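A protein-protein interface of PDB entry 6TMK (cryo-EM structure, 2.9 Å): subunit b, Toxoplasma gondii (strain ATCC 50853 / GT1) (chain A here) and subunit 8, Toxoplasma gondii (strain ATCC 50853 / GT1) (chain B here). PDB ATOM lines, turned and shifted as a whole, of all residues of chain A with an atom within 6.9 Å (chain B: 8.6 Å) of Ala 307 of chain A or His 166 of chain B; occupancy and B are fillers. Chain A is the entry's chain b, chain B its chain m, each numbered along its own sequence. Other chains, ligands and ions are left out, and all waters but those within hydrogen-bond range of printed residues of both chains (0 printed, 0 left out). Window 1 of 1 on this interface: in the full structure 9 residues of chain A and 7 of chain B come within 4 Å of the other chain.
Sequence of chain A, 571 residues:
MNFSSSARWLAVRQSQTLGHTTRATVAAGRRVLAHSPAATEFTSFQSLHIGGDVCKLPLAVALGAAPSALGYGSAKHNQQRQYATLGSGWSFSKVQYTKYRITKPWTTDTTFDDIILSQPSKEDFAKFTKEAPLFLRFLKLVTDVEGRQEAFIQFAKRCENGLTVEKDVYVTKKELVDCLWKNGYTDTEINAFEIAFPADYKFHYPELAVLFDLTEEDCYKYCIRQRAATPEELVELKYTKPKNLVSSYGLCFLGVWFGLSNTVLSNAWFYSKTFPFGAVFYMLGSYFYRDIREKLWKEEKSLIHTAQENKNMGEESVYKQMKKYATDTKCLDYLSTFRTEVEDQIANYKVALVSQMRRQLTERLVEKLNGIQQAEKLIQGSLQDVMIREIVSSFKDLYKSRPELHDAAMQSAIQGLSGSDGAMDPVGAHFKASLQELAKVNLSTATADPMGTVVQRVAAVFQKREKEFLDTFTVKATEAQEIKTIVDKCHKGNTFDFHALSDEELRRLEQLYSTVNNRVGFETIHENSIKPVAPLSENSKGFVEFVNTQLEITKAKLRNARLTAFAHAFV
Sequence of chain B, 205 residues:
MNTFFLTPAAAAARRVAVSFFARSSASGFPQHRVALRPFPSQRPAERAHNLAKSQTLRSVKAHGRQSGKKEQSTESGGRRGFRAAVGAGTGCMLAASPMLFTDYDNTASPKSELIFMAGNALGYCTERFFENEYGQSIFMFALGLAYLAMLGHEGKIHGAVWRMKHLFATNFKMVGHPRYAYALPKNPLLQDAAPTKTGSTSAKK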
ATOM      1  N   TRP A  90      -7.059  -2.527 -32.079  1.00  0.00           N
ATOM      2  CA  TRP A  90      -8.159  -1.888 -31.377  1.00  0.00           C
ATOM      3  C   TRP A  90      -7.898  -0.416 -31.101  1.00  0.00           C
ATOM      4  O   TRP A  90      -8.686   0.222 -30.398  1.00  0.00           O
ATOM      5  CB  TRP A  90      -8.429  -2.620 -30.065  1.00  0.00           C
ATOM      6  CG  TRP A  90      -9.324  -3.792 -30.202  1.00  0.00           C
ATOM      7  CD1 TRP A  90      -8.963  -5.059 -30.529  1.00  0.00           C
ATOM      8  CD2 TRP A  90     -10.736  -3.813 -30.003  1.00  0.00           C
ATOM      9  NE1 TRP A  90     -10.066  -5.870 -30.555  1.00  0.00           N
ATOM     10  CE2 TRP A  90     -11.168  -5.128 -30.232  1.00  0.00           C
ATOM     11  CE3 TRP A  90     -11.679  -2.847 -29.655  1.00  0.00           C
ATOM     12  CZ2 TRP A  90     -12.498  -5.501 -30.127  1.00  0.00           C
ATOM     13  CZ3 TRP A  90     -12.994  -3.218 -29.554  1.00  0.00           C
ATOM     14  CH2 TRP A  90     -13.394  -4.533 -29.785  1.00  0.00           C
ATOM     15  N   GLU A 300     -17.810   7.805 -30.059  1.00  0.00           N
ATOM     16  CA  GLU A 300     -17.144   6.659 -30.662  1.00  0.00           C
ATOM     17  C   GLU A 300     -16.018   6.147 -29.775  1.00  0.00           C
ATOM     18  O   GLU A 300     -15.854   4.932 -29.604  1.00  0.00           O
ATOM     19  CB  GLU A 300     -16.613   7.042 -32.040  1.00  0.00           C
ATOM     20  CG  GLU A 300     -15.936   5.913 -32.771  1.00  0.00           C
ATOM     21  CD  GLU A 300     -16.128   5.986 -34.271  1.00  0.00           C
ATOM     22  OE1 GLU A 300     -16.323   7.104 -34.792  1.00  0.00           O
ATOM     23  OE2 GLU A 300     -16.083   4.925 -34.927  1.00  0.00           O
ATOM     24  N   SER A 302     -15.775   6.422 -26.502  1.00  0.00           N
ATOM     25  CA  SER A 302     -16.365   5.767 -25.340  1.00  0.00           C
ATOM     26  C   SER A 302     -16.896   4.386 -25.695  1.00  0.00           C
ATOM     27  O   SER A 302     -16.725   3.427 -24.931  1.00  0.00           O
ATOM     28  CB  SER A 302     -17.475   6.639 -24.767  1.00  0.00           C
ATOM     29  OG  SER A 302     -18.646   6.551 -25.552  1.00  0.00           O
ATOM     30  N   LEU A 303     -17.535   4.261 -26.857  1.00  0.00           N
ATOM     31  CA  LEU A 303     -18.081   2.974 -27.266  1.00  0.00           C
ATOM     32  C   LEU A 303     -16.974   1.953 -27.485  1.00  0.00           C
ATOM     33  O   LEU A 303     -17.099   0.791 -27.079  1.00  0.00           O
ATOM     34  CB  LEU A 303     -18.899   3.137 -28.541  1.00  0.00           C
ATOM     35  CG  LEU A 303     -20.216   3.897 -28.469  1.00  0.00           C
ATOM     36  CD1 LEU A 303     -20.777   4.028 -29.856  1.00  0.00           C
ATOM     37  CD2 LEU A 303     -21.203   3.215 -27.573  1.00  0.00           C
ATOM     38  N   ILE A 304     -15.890   2.365 -28.140  1.00  0.00           N
ATOM     39  CA  ILE A 304     -14.783   1.449 -28.393  1.00  0.00           C
ATOM     40  C   ILE A 304     -14.157   1.001 -27.080  1.00  0.00           C
ATOM     41  O   ILE A 304     -13.832  -0.182 -26.896  1.00  0.00           O
ATOM     42  CB  ILE A 304     -13.764   2.123 -29.329  1.00  0.00           C
ATOM     43  CG1 ILE A 304     -14.348   2.227 -30.733  1.00  0.00           C
ATOM     44  CG2 ILE A 304     -12.474   1.359 -29.374  1.00  0.00           C
ATOM     45  CD1 ILE A 304     -13.806   3.347 -31.539  1.00  0.00           C
ATOM     46  N   HIS A 305     -13.997   1.932 -26.139  1.00  0.00           N
ATOM     47  CA  HIS A 305     -13.483   1.582 -24.820  1.00  0.00           C
ATOM     48  C   HIS A 305     -14.372   0.546 -24.141  1.00  0.00           C
ATOM     49  O   HIS A 305     -13.887  -0.469 -23.622  1.00  0.00           O
ATOM     50  CB  HIS A 305     -13.373   2.846 -23.973  1.00  0.00           C
ATOM     51  CG  HIS A 305     -12.837   2.612 -22.598  1.00  0.00           C
ATOM     52  ND1 HIS A 305     -13.620   2.138 -21.568  1.00  0.00           N
ATOM     53  CD2 HIS A 305     -11.602   2.798 -22.078  1.00  0.00           C
ATOM     54  CE1 HIS A 305     -12.888   2.035 -20.475  1.00  0.00           C
ATOM     55  NE2 HIS A 305     -11.659   2.428 -20.757  1.00  0.00           N
ATOM     56  N   THR A 306     -15.682   0.796 -24.131  1.00  0.00           N
ATOM     57  CA  THR A 306     -16.619  -0.130 -23.503  1.00  0.00           C
ATOM     58  C   THR A 306     -16.538  -1.512 -24.131  1.00  0.00           C
ATOM     59  O   THR A 306     -16.519  -2.529 -23.424  1.00  0.00           O
ATOM     60  CB  THR A 306     -18.036   0.428 -23.610  1.00  0.00           C
ATOM     61  OG1 THR A 306     -18.173   1.574 -22.763  1.00  0.00           O
ATOM     62  CG2 THR A 306     -19.059  -0.609 -23.232  1.00  0.00           C
ATOM     63  N   ALA A 307     -16.490  -1.571 -25.460  1.00  0.00           N
ATOM     64  CA  ALA A 307     -16.442  -2.856 -26.147  1.00  0.00           C
ATOM     65  C   ALA A 307     -15.182  -3.624 -25.780  1.00  0.00           C
ATOM     66  O   ALA A 307     -15.234  -4.825 -25.487  1.00  0.00           O
ATOM     67  CB  ALA A 307     -16.518  -2.635 -27.652  1.00  0.00           C
ATOM     68  N   GLN A 308     -14.037  -2.944 -25.796  1.00  0.00           N
ATOM     69  CA  GLN A 308     -12.787  -3.618 -25.467  1.00  0.00           C
ATOM     70  C   GLN A 308     -12.804  -4.135 -24.035  1.00  0.00           C
ATOM     71  O   GLN A 308     -12.355  -5.257 -23.768  1.00  0.00           O
ATOM     72  CB  GLN A 308     -11.612  -2.673 -25.688  1.00  0.00           C
ATOM     73  CG  GLN A 308     -10.276  -3.373 -25.739  1.00  0.00           C
ATOM     74  CD  GLN A 308      -9.166  -2.478 -26.229  1.00  0.00           C
ATOM     75  OE1 GLN A 308      -9.226  -1.257 -26.083  1.00  0.00           O
ATOM     76  NE2 GLN A 308      -8.145  -3.078 -26.823  1.00  0.00           N
ATOM     77  N   GLU A 309     -13.334  -3.345 -23.099  1.00  0.00           N
ATOM     78  CA  GLU A 309     -13.360  -3.791 -21.710  1.00  0.00           C
ATOM     79  C   GLU A 309     -14.265  -5.002 -21.537  1.00  0.00           C
ATOM     80  O   GLU A 309     -13.917  -5.951 -20.819  1.00  0.00           O
ATOM     81  CB  GLU A 309     -13.829  -2.659 -20.802  1.00  0.00           C
ATOM     82  CG  GLU A 309     -12.912  -1.459 -20.766  1.00  0.00           C
ATOM     83  CD  GLU A 309     -11.602  -1.738 -20.055  1.00  0.00           C
ATOM     84  OE1 GLU A 309     -11.557  -2.670 -19.226  1.00  0.00           O
ATOM     85  OE2 GLU A 309     -10.614  -1.023 -20.329  1.00  0.00           O
ATOM     86  N   ASN A 310     -15.436  -4.981 -22.173  1.00  0.00           N
ATOM     87  CA  ASN A 310     -16.341  -6.121 -22.089  1.00  0.00           C
ATOM     88  C   ASN A 310     -15.678  -7.378 -22.629  1.00  0.00           C
ATOM     89  O   ASN A 310     -15.724  -8.448 -22.001  1.00  0.00           O
ATOM     90  CB  ASN A 310     -17.621  -5.820 -22.861  1.00  0.00           C
ATOM     91  CG  ASN A 310     -18.493  -4.804 -22.169  1.00  0.00           C
ATOM     92  OD1 ASN A 310     -18.235  -4.411 -21.034  1.00  0.00           O
ATOM     93  ND2 ASN A 310     -19.537  -4.367 -22.856  1.00  0.00           N
ATOM     94  N   LYS A 311     -15.040  -7.261 -23.793  1.00  0.00           N
ATOM     95  CA  LYS A 311     -14.331  -8.389 -24.381  1.00  0.00           C
ATOM     96  C   LYS A 311     -13.283  -8.937 -23.424  1.00  0.00           C
ATOM     97  O   LYS A 311     -13.212 -10.152 -23.186  1.00  0.00           O
ATOM     98  CB  LYS A 311     -13.694  -7.945 -25.692  1.00  0.00           C
ATOM     99  CG  LYS A 311     -13.146  -9.044 -26.556  1.00  0.00           C
ATOM    100  CD  LYS A 311     -12.087  -8.493 -27.480  1.00  0.00           C
ATOM    101  CE  LYS A 311     -11.442  -9.571 -28.317  1.00  0.00           C
ATOM    102  NZ  LYS A 311     -12.311  -9.985 -29.437  1.00  0.00           N
ATOM    103  N   ASN A 312     -12.460  -8.053 -22.861  1.00  0.00           N
ATOM    104  CA  ASN A 312     -11.384  -8.501 -21.985  1.00  0.00           C
ATOM    105  C   ASN A 312     -11.929  -9.235 -20.770  1.00  0.00           C
ATOM    106  O   ASN A 312     -11.464 -10.333 -20.432  1.00  0.00           O
ATOM    107  CB  ASN A 312     -10.527  -7.314 -21.550  1.00  0.00           C
ATOM    108  CG  ASN A 312      -9.869  -6.603 -22.712  1.00  0.00           C
ATOM    109  OD1 ASN A 312      -9.866  -5.376 -22.778  1.00  0.00           O
ATOM    110  ND2 ASN A 312      -9.300  -7.369 -23.629  1.00  0.00           N
ATOM    111  N   HIS B 158     -29.756   3.621 -38.150  1.00  0.00           N
ATOM    112  CA  HIS B 158     -28.320   3.431 -38.302  1.00  0.00           C
ATOM    113  C   HIS B 158     -27.600   3.671 -36.984  1.00  0.00           C
ATOM    114  O   HIS B 158     -26.756   2.872 -36.573  1.00  0.00           O
ATOM    115  CB  HIS B 158     -27.787   4.364 -39.384  1.00  0.00           C
ATOM    116  CG  HIS B 158     -26.426   3.998 -39.879  1.00  0.00           C
ATOM    117  ND1 HIS B 158     -25.336   3.883 -39.047  1.00  0.00           N
ATOM    118  CD2 HIS B 158     -25.974   3.734 -41.128  1.00  0.00           C
ATOM    119  CE1 HIS B 158     -24.276   3.549 -39.757  1.00  0.00           C
ATOM    120  NE2 HIS B 158     -24.636   3.456 -41.024  1.00  0.00           N
ATOM    121  N   GLY B 159     -27.909   4.782 -36.322  1.00  0.00           N
ATOM    122  CA  GLY B 159     -27.291   5.063 -35.038  1.00  0.00           C
ATOM    123  C   GLY B 159     -27.605   4.004 -34.002  1.00  0.00           C
ATOM    124  O   GLY B 159     -26.730   3.585 -33.238  1.00  0.00           O
ATOM    125  N   ALA B 160     -28.857   3.552 -33.967  1.00  0.00           N
ATOM    126  CA  ALA B 160     -29.246   2.530 -33.005  1.00  0.00           C
ATOM    127  C   ALA B 160     -28.443   1.254 -33.211  1.00  0.00           C
ATOM    128  O   ALA B 160     -27.921   0.678 -32.253  1.00  0.00           O
ATOM    129  CB  ALA B 160     -30.739   2.245 -33.118  1.00  0.00           C
ATOM    130  N   VAL B 161     -28.334   0.794 -34.457  1.00  0.00           N
ATOM    131  CA  VAL B 161     -27.594  -0.435 -34.718  1.00  0.00           C
ATOM    132  C   VAL B 161     -26.108  -0.231 -34.470  1.00  0.00           C
ATOM    133  O   VAL B 161     -25.412  -1.142 -34.008  1.00  0.00           O
ATOM    134  CB  VAL B 161     -27.860  -0.922 -36.152  1.00  0.00           C
ATOM    135  CG1 VAL B 161     -27.098  -2.192 -36.425  1.00  0.00           C
ATOM    136  CG2 VAL B 161     -29.319  -1.156 -36.369  1.00  0.00           C
ATOM    137  N   TRP B 162     -25.594   0.955 -34.784  1.00  0.00           N
ATOM    138  CA  TRP B 162     -24.185   1.243 -34.584  1.00  0.00           C
ATOM    139  C   TRP B 162     -23.815   1.229 -33.109  1.00  0.00           C
ATOM    140  O   TRP B 162     -22.686   0.871 -32.757  1.00  0.00           O
ATOM    141  CB  TRP B 162     -23.861   2.587 -35.226  1.00  0.00           C
ATOM    142  CG  TRP B 162     -22.480   3.060 -35.028  1.00  0.00           C
ATOM    143  CD1 TRP B 162     -21.358   2.563 -35.603  1.00  0.00           C
ATOM    144  CD2 TRP B 162     -22.065   4.148 -34.208  1.00  0.00           C
ATOM    145  NE1 TRP B 162     -20.263   3.267 -35.186  1.00  0.00           N
ATOM    146  CE2 TRP B 162     -20.672   4.250 -34.326  1.00  0.00           C
ATOM    147  CE3 TRP B 162     -22.737   5.047 -33.380  1.00  0.00           C
ATOM    148  CZ2 TRP B 162     -19.938   5.210 -33.648  1.00  0.00           C
ATOM    149  CZ3 TRP B 162     -22.008   5.997 -32.711  1.00  0.00           C
ATOM    150  CH2 TRP B 162     -20.623   6.072 -32.847  1.00  0.00           C
ATOM    151  N   ARG B 163     -24.748   1.605 -32.238  1.00  0.00           N
ATOM    152  CA  ARG B 163     -24.508   1.500 -30.803  1.00  0.00           C
ATOM    153  C   ARG B 163     -24.735   0.079 -30.301  1.00  0.00           C
ATOM    154  O   ARG B 163     -24.001  -0.399 -29.426  1.00  0.00           O
ATOM    155  CB  ARG B 163     -25.403   2.478 -30.051  1.00  0.00           C
ATOM    156  CG  ARG B 163     -25.089   3.916 -30.350  1.00  0.00           C
ATOM    157  CD  ARG B 163     -25.957   4.881 -29.589  1.00  0.00           C
ATOM    158  NE  ARG B 163     -25.623   6.255 -29.945  1.00  0.00           N
ATOM    159  CZ  ARG B 163     -26.283   6.988 -30.834  1.00  0.00           C
ATOM    160  NH1 ARG B 163     -27.340   6.503 -31.463  1.00  0.00           N
ATOM    161  NH2 ARG B 163     -25.882   8.218 -31.097  1.00  0.00           N
ATOM    162  N   MET B 164     -25.759  -0.594 -30.827  1.00  0.00           N
ATOM    163  CA  MET B 164     -26.007  -1.984 -30.474  1.00  0.00           C
ATOM    164  C   MET B 164     -24.777  -2.833 -30.727  1.00  0.00           C
ATOM    165  O   MET B 164     -24.426  -3.690 -29.915  1.00  0.00           O
ATOM    166  CB  MET B 164     -27.184  -2.529 -31.275  1.00  0.00           C
ATOM    167  CG  MET B 164     -28.521  -2.217 -30.695  1.00  0.00           C
ATOM    168  SD  MET B 164     -29.874  -2.837 -31.699  1.00  0.00           S
ATOM    169  CE  MET B 164     -31.142  -1.660 -31.252  1.00  0.00           C
ATOM    170  N   LYS B 165     -24.114  -2.615 -31.856  1.00  0.00           N
ATOM    171  CA  LYS B 165     -22.905  -3.360 -32.164  1.00  0.00           C
ATOM    172  C   LYS B 165     -21.908  -3.251 -31.021  1.00  0.00           C
ATOM    173  O   LYS B 165     -21.580  -4.243 -30.360  1.00  0.00           O
ATOM    174  CB  LYS B 165     -22.310  -2.826 -33.462  1.00  0.00           C
ATOM    175  CG  LYS B 165     -21.075  -3.518 -33.932  1.00  0.00           C
ATOM    176  CD  LYS B 165     -20.714  -3.074 -35.325  1.00  0.00           C
ATOM    177  CE  LYS B 165     -20.162  -1.676 -35.327  1.00  0.00           C
ATOM    178  NZ  LYS B 165     -19.482  -1.347 -36.593  1.00  0.00           N
ATOM    179  N   HIS B 166     -21.478  -2.027 -30.727  1.00  0.00           N
ATOM    180  CA  HIS B 166     -20.432  -1.820 -29.741  1.00  0.00           C
ATOM    181  C   HIS B 166     -20.843  -2.310 -28.361  1.00  0.00           C
ATOM    182  O   HIS B 166     -19.999  -2.808 -27.610  1.00  0.00           O
ATOM    183  CB  HIS B 166     -20.071  -0.342 -29.686  1.00  0.00           C
ATOM    184  CG  HIS B 166     -19.302   0.138 -30.875  1.00  0.00           C
ATOM    185  ND1 HIS B 166     -19.911   0.655 -31.996  1.00  0.00           N
ATOM    186  CD2 HIS B 166     -17.971   0.199 -31.108  1.00  0.00           C
ATOM    187  CE1 HIS B 166     -18.989   0.999 -32.874  1.00  0.00           C
ATOM    188  NE2 HIS B 166     -17.804   0.737 -32.359  1.00  0.00           N
ATOM    189  N   LEU B 167     -22.119  -2.182 -28.000  1.00  0.00           N
ATOM    190  CA  LEU B 167     -22.528  -2.449 -26.630  1.00  0.00           C
ATOM    191  C   LEU B 167     -23.066  -3.854 -26.403  1.00  0.00           C
ATOM    192  O   LEU B 167     -23.232  -4.249 -25.245  1.00  0.00           O
ATOM    193  CB  LEU B 167     -23.593  -1.444 -26.197  1.00  0.00           C
ATOM    194  CG  LEU B 167     -23.217   0.028 -26.263  1.00  0.00           C
ATOM    195  CD1 LEU B 167     -24.326   0.840 -25.678  1.00  0.00           C
ATOM    196  CD2 LEU B 167     -21.929   0.282 -25.529  1.00  0.00           C
ATOM    197  N   PHE B 168     -23.336  -4.619 -27.455  1.00  0.00           N
ATOM    198  CA  PHE B 168     -23.857  -5.968 -27.322  1.00  0.00           C
ATOM    199  C   PHE B 168     -22.962  -7.048 -27.897  1.00  0.00           C
ATOM    200  O   PHE B 168     -23.028  -8.184 -27.427  1.00  0.00           O
ATOM    201  CB  PHE B 168     -25.229  -6.087 -28.003  1.00  0.00           C
ATOM    202  CG  PHE B 168     -26.308  -5.247 -27.382  1.00  0.00           C
ATOM    203  CD1 PHE B 168     -26.140  -4.658 -26.148  1.00  0.00           C
ATOM    204  CD2 PHE B 168     -27.503  -5.059 -28.043  1.00  0.00           C
ATOM    205  CE1 PHE B 168     -27.139  -3.898 -25.590  1.00  0.00           C
ATOM    206  CE2 PHE B 168     -28.503  -4.302 -27.489  1.00  0.00           C
ATOM    207  CZ  PHE B 168     -28.322  -3.721 -26.261  1.00  0.00           C
ATOM    208  N   ALA B 169     -22.134  -6.745 -28.896  1.00  0.00           N
ATOM    209  CA  ALA B 169     -21.484  -7.797 -29.655  1.00  0.00           C
ATOM    210  C   ALA B 169     -20.274  -8.392 -28.950  1.00  0.00           C
ATOM    211  O   ALA B 169     -19.727  -9.385 -29.440  1.00  0.00           O
ATOM    212  CB  ALA B 169     -21.066  -7.253 -31.019  1.00  0.00           C
ATOM    213  N   THR B 170     -19.844  -7.823 -27.823  1.00  0.00           N
ATOM    214  CA  THR B 170     -18.624  -8.268 -27.158  1.00  0.00           C
ATOM    215  C   THR B 170     -18.811  -8.377 -25.650  1.00  0.00           C
ATOM    216  O   THR B 170     -17.862  -8.168 -24.891  1.00  0.00           O
ATOM    217  CB  THR B 170     -17.469  -7.323 -27.459  1.00  0.00           C
ATOM    218  OG1 THR B 170     -17.904  -5.972 -27.280  1.00  0.00           O
ATOM    219  CG2 THR B 170     -16.995  -7.510 -28.866  1.00  0.00           C
ATOM    220  N   ASN B 171     -20.014  -8.714 -25.203  1.00  0.00           N
ATOM    221  CA  ASN B 171     -20.339  -8.730 -23.784  1.00  0.00           C
ATOM    222  C   ASN B 171     -20.097 -10.095 -23.147  1.00  0.00           C
ATOM    223  O   ASN B 171     -19.530 -10.177 -22.054  1.00  0.00           O
ATOM    224  CB  ASN B 171     -21.787  -8.297 -23.578  1.00  0.00           C
ATOM    225  CG  ASN B 171     -22.042  -7.782 -22.185  1.00  0.00           C
ATOM    226  OD1 ASN B 171     -21.598  -8.369 -21.201  1.00  0.00           O
ATOM    227  ND2 ASN B 171     -22.751  -6.673 -22.093  1.00  0.00           N
ATOM    228  N   PHE B 172     -20.532 -11.163 -23.818  1.00  0.00           N
ATOM    229  CA  PHE B 172     -20.573 -12.526 -23.290  1.00  0.00           C
ATOM    230  C   PHE B 172     -21.694 -12.699 -22.274  1.00  0.00           C
ATOM    231  O   PHE B 172     -21.971 -13.822 -21.841  1.00  0.00           O
ATOM    232  CB  PHE B 172     -19.250 -12.931 -22.631  1.00  0.00           C
ATOM    233  CG  PHE B 172     -18.082 -12.962 -23.558  1.00  0.00           C
ATOM    234  CD1 PHE B 172     -17.621 -14.160 -24.057  1.00  0.00           C
ATOM    235  CD2 PHE B 172     -17.424 -11.802 -23.909  1.00  0.00           C
ATOM    236  CE1 PHE B 172     -16.540 -14.202 -24.900  1.00  0.00           C
ATOM    237  CE2 PHE B 172     -16.347 -11.838 -24.755  1.00  0.00           C
ATOM    238  CZ  PHE B 172     -15.903 -13.042 -25.249  1.00  0.00           C
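The side-chain hydroxyl (OG1) of Thr 170 of chain B is in hydrogen-bond range of the backbone carbonyl oxygen (O) of Ala 307 of chain A, 3.4 Å away.
O of Thr 170 of chain B is in hydrogen-bond range of N of Lys 311 of chain A (3.2 Å).
The backbone carbonyl oxygen (O) of Ser 302 of chain A is in hydrogen-bond range of the side-chain hydroxyl (OG1) of Thr 306 of chain A (3.2 Å).
O of Thr 306 of chain A lies close to OD1 of Asn 310 of chain A (3.5 Å).
A ring nitrogen (ND1) of His 166 of chain B lies within hydrogen-bond range of the backbone carbonyl oxygen (O) of Trp 162 of chain B (2.9 Å).
Glu 300 of chain A touches Trp 162 of chain B (CD to CZ2, 3.9 Å).
Trp 162 of chain B touches Leu 303 of chain A.
His 166 of chain B touches Leu 303 of chain A (CG to CB, 3.8 Å).
Leu 303 of chain A touches Leu 167 of chain B.
Thr 306 of chain A touches Leu 167 of chain B (CG2 to CD2, 3.8 Å).
Ala 307 of chain A touches His 166 of chain B.
Thr 170 of chain B touches Asn 310 of chain A (O to CB, 3.1 Å).
Lys 311 of chain A touches Phe 172 of chain B (O to CE2, 3.9 Å).
Thr 306 of chain A touches just one residue of chain B: Leu 167 (3.8 Å).
Ala 307 of chain A touches just these residues of chain B: His 166 and Thr 170.
Printed residues of chain B within 4 Å of Asn 310 of chain A: Thr 170 (3.1 Å).
Printed residues of chain A within 4 Å of Trp 162 of chain B: Glu 300 and Leu 303.
Of chain A, only Leu 303 (3.8 Å) and Ala 307 (3.5 Å) come within 4 Å of His 166 of chain B.
Of the printed residues of chain A, Leu 167 of chain B touches Leu 303 and Thr 306.
Printed residues of chain A within 4 Å of Thr 170 of chain B: Ala 307 (3.4 Å), Asn 310 (3.1 Å) and Lys 311 (3.2 Å).
The nearest residue of chain B that does not touch Ala 307 of chain A is Leu 167 of chain B (5.6 Å).
The nearest residue of chain A that does not touch His 166 of chain B is Ile 304 of chain A (4.1 Å).
The nearest printed residue of chain A that does not touch Thr 170 of chain B is Trp 90 of chain A (4.8 Å).
Of the 13 printed residues of chain A, 6 touch a printed residue of chain B.
Hydrophobic or aromatic side chains of chain A that line the printed part of chain B: Leu 303 and Ala 307.
Of the 15 printed residues of chain B, 5 touch a printed residue of chain A.
Printed residues of chain B that touch a printed residue of chain A: Trp 162, His 166, Leu 167, Thr 170 and Phe 172.
Hydrophobic or aromatic side chains of chain B within 4 Å of the printed part of chain A: Trp 162, His 166, Leu 167 and Phe 172.
Among the printed residues, 10 pairs touch across the chains.
Among the printed residues, no Asp or Glu carboxylate lies within 4 Å of a Lys or Arg side-chain nitrogen of the other chain.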
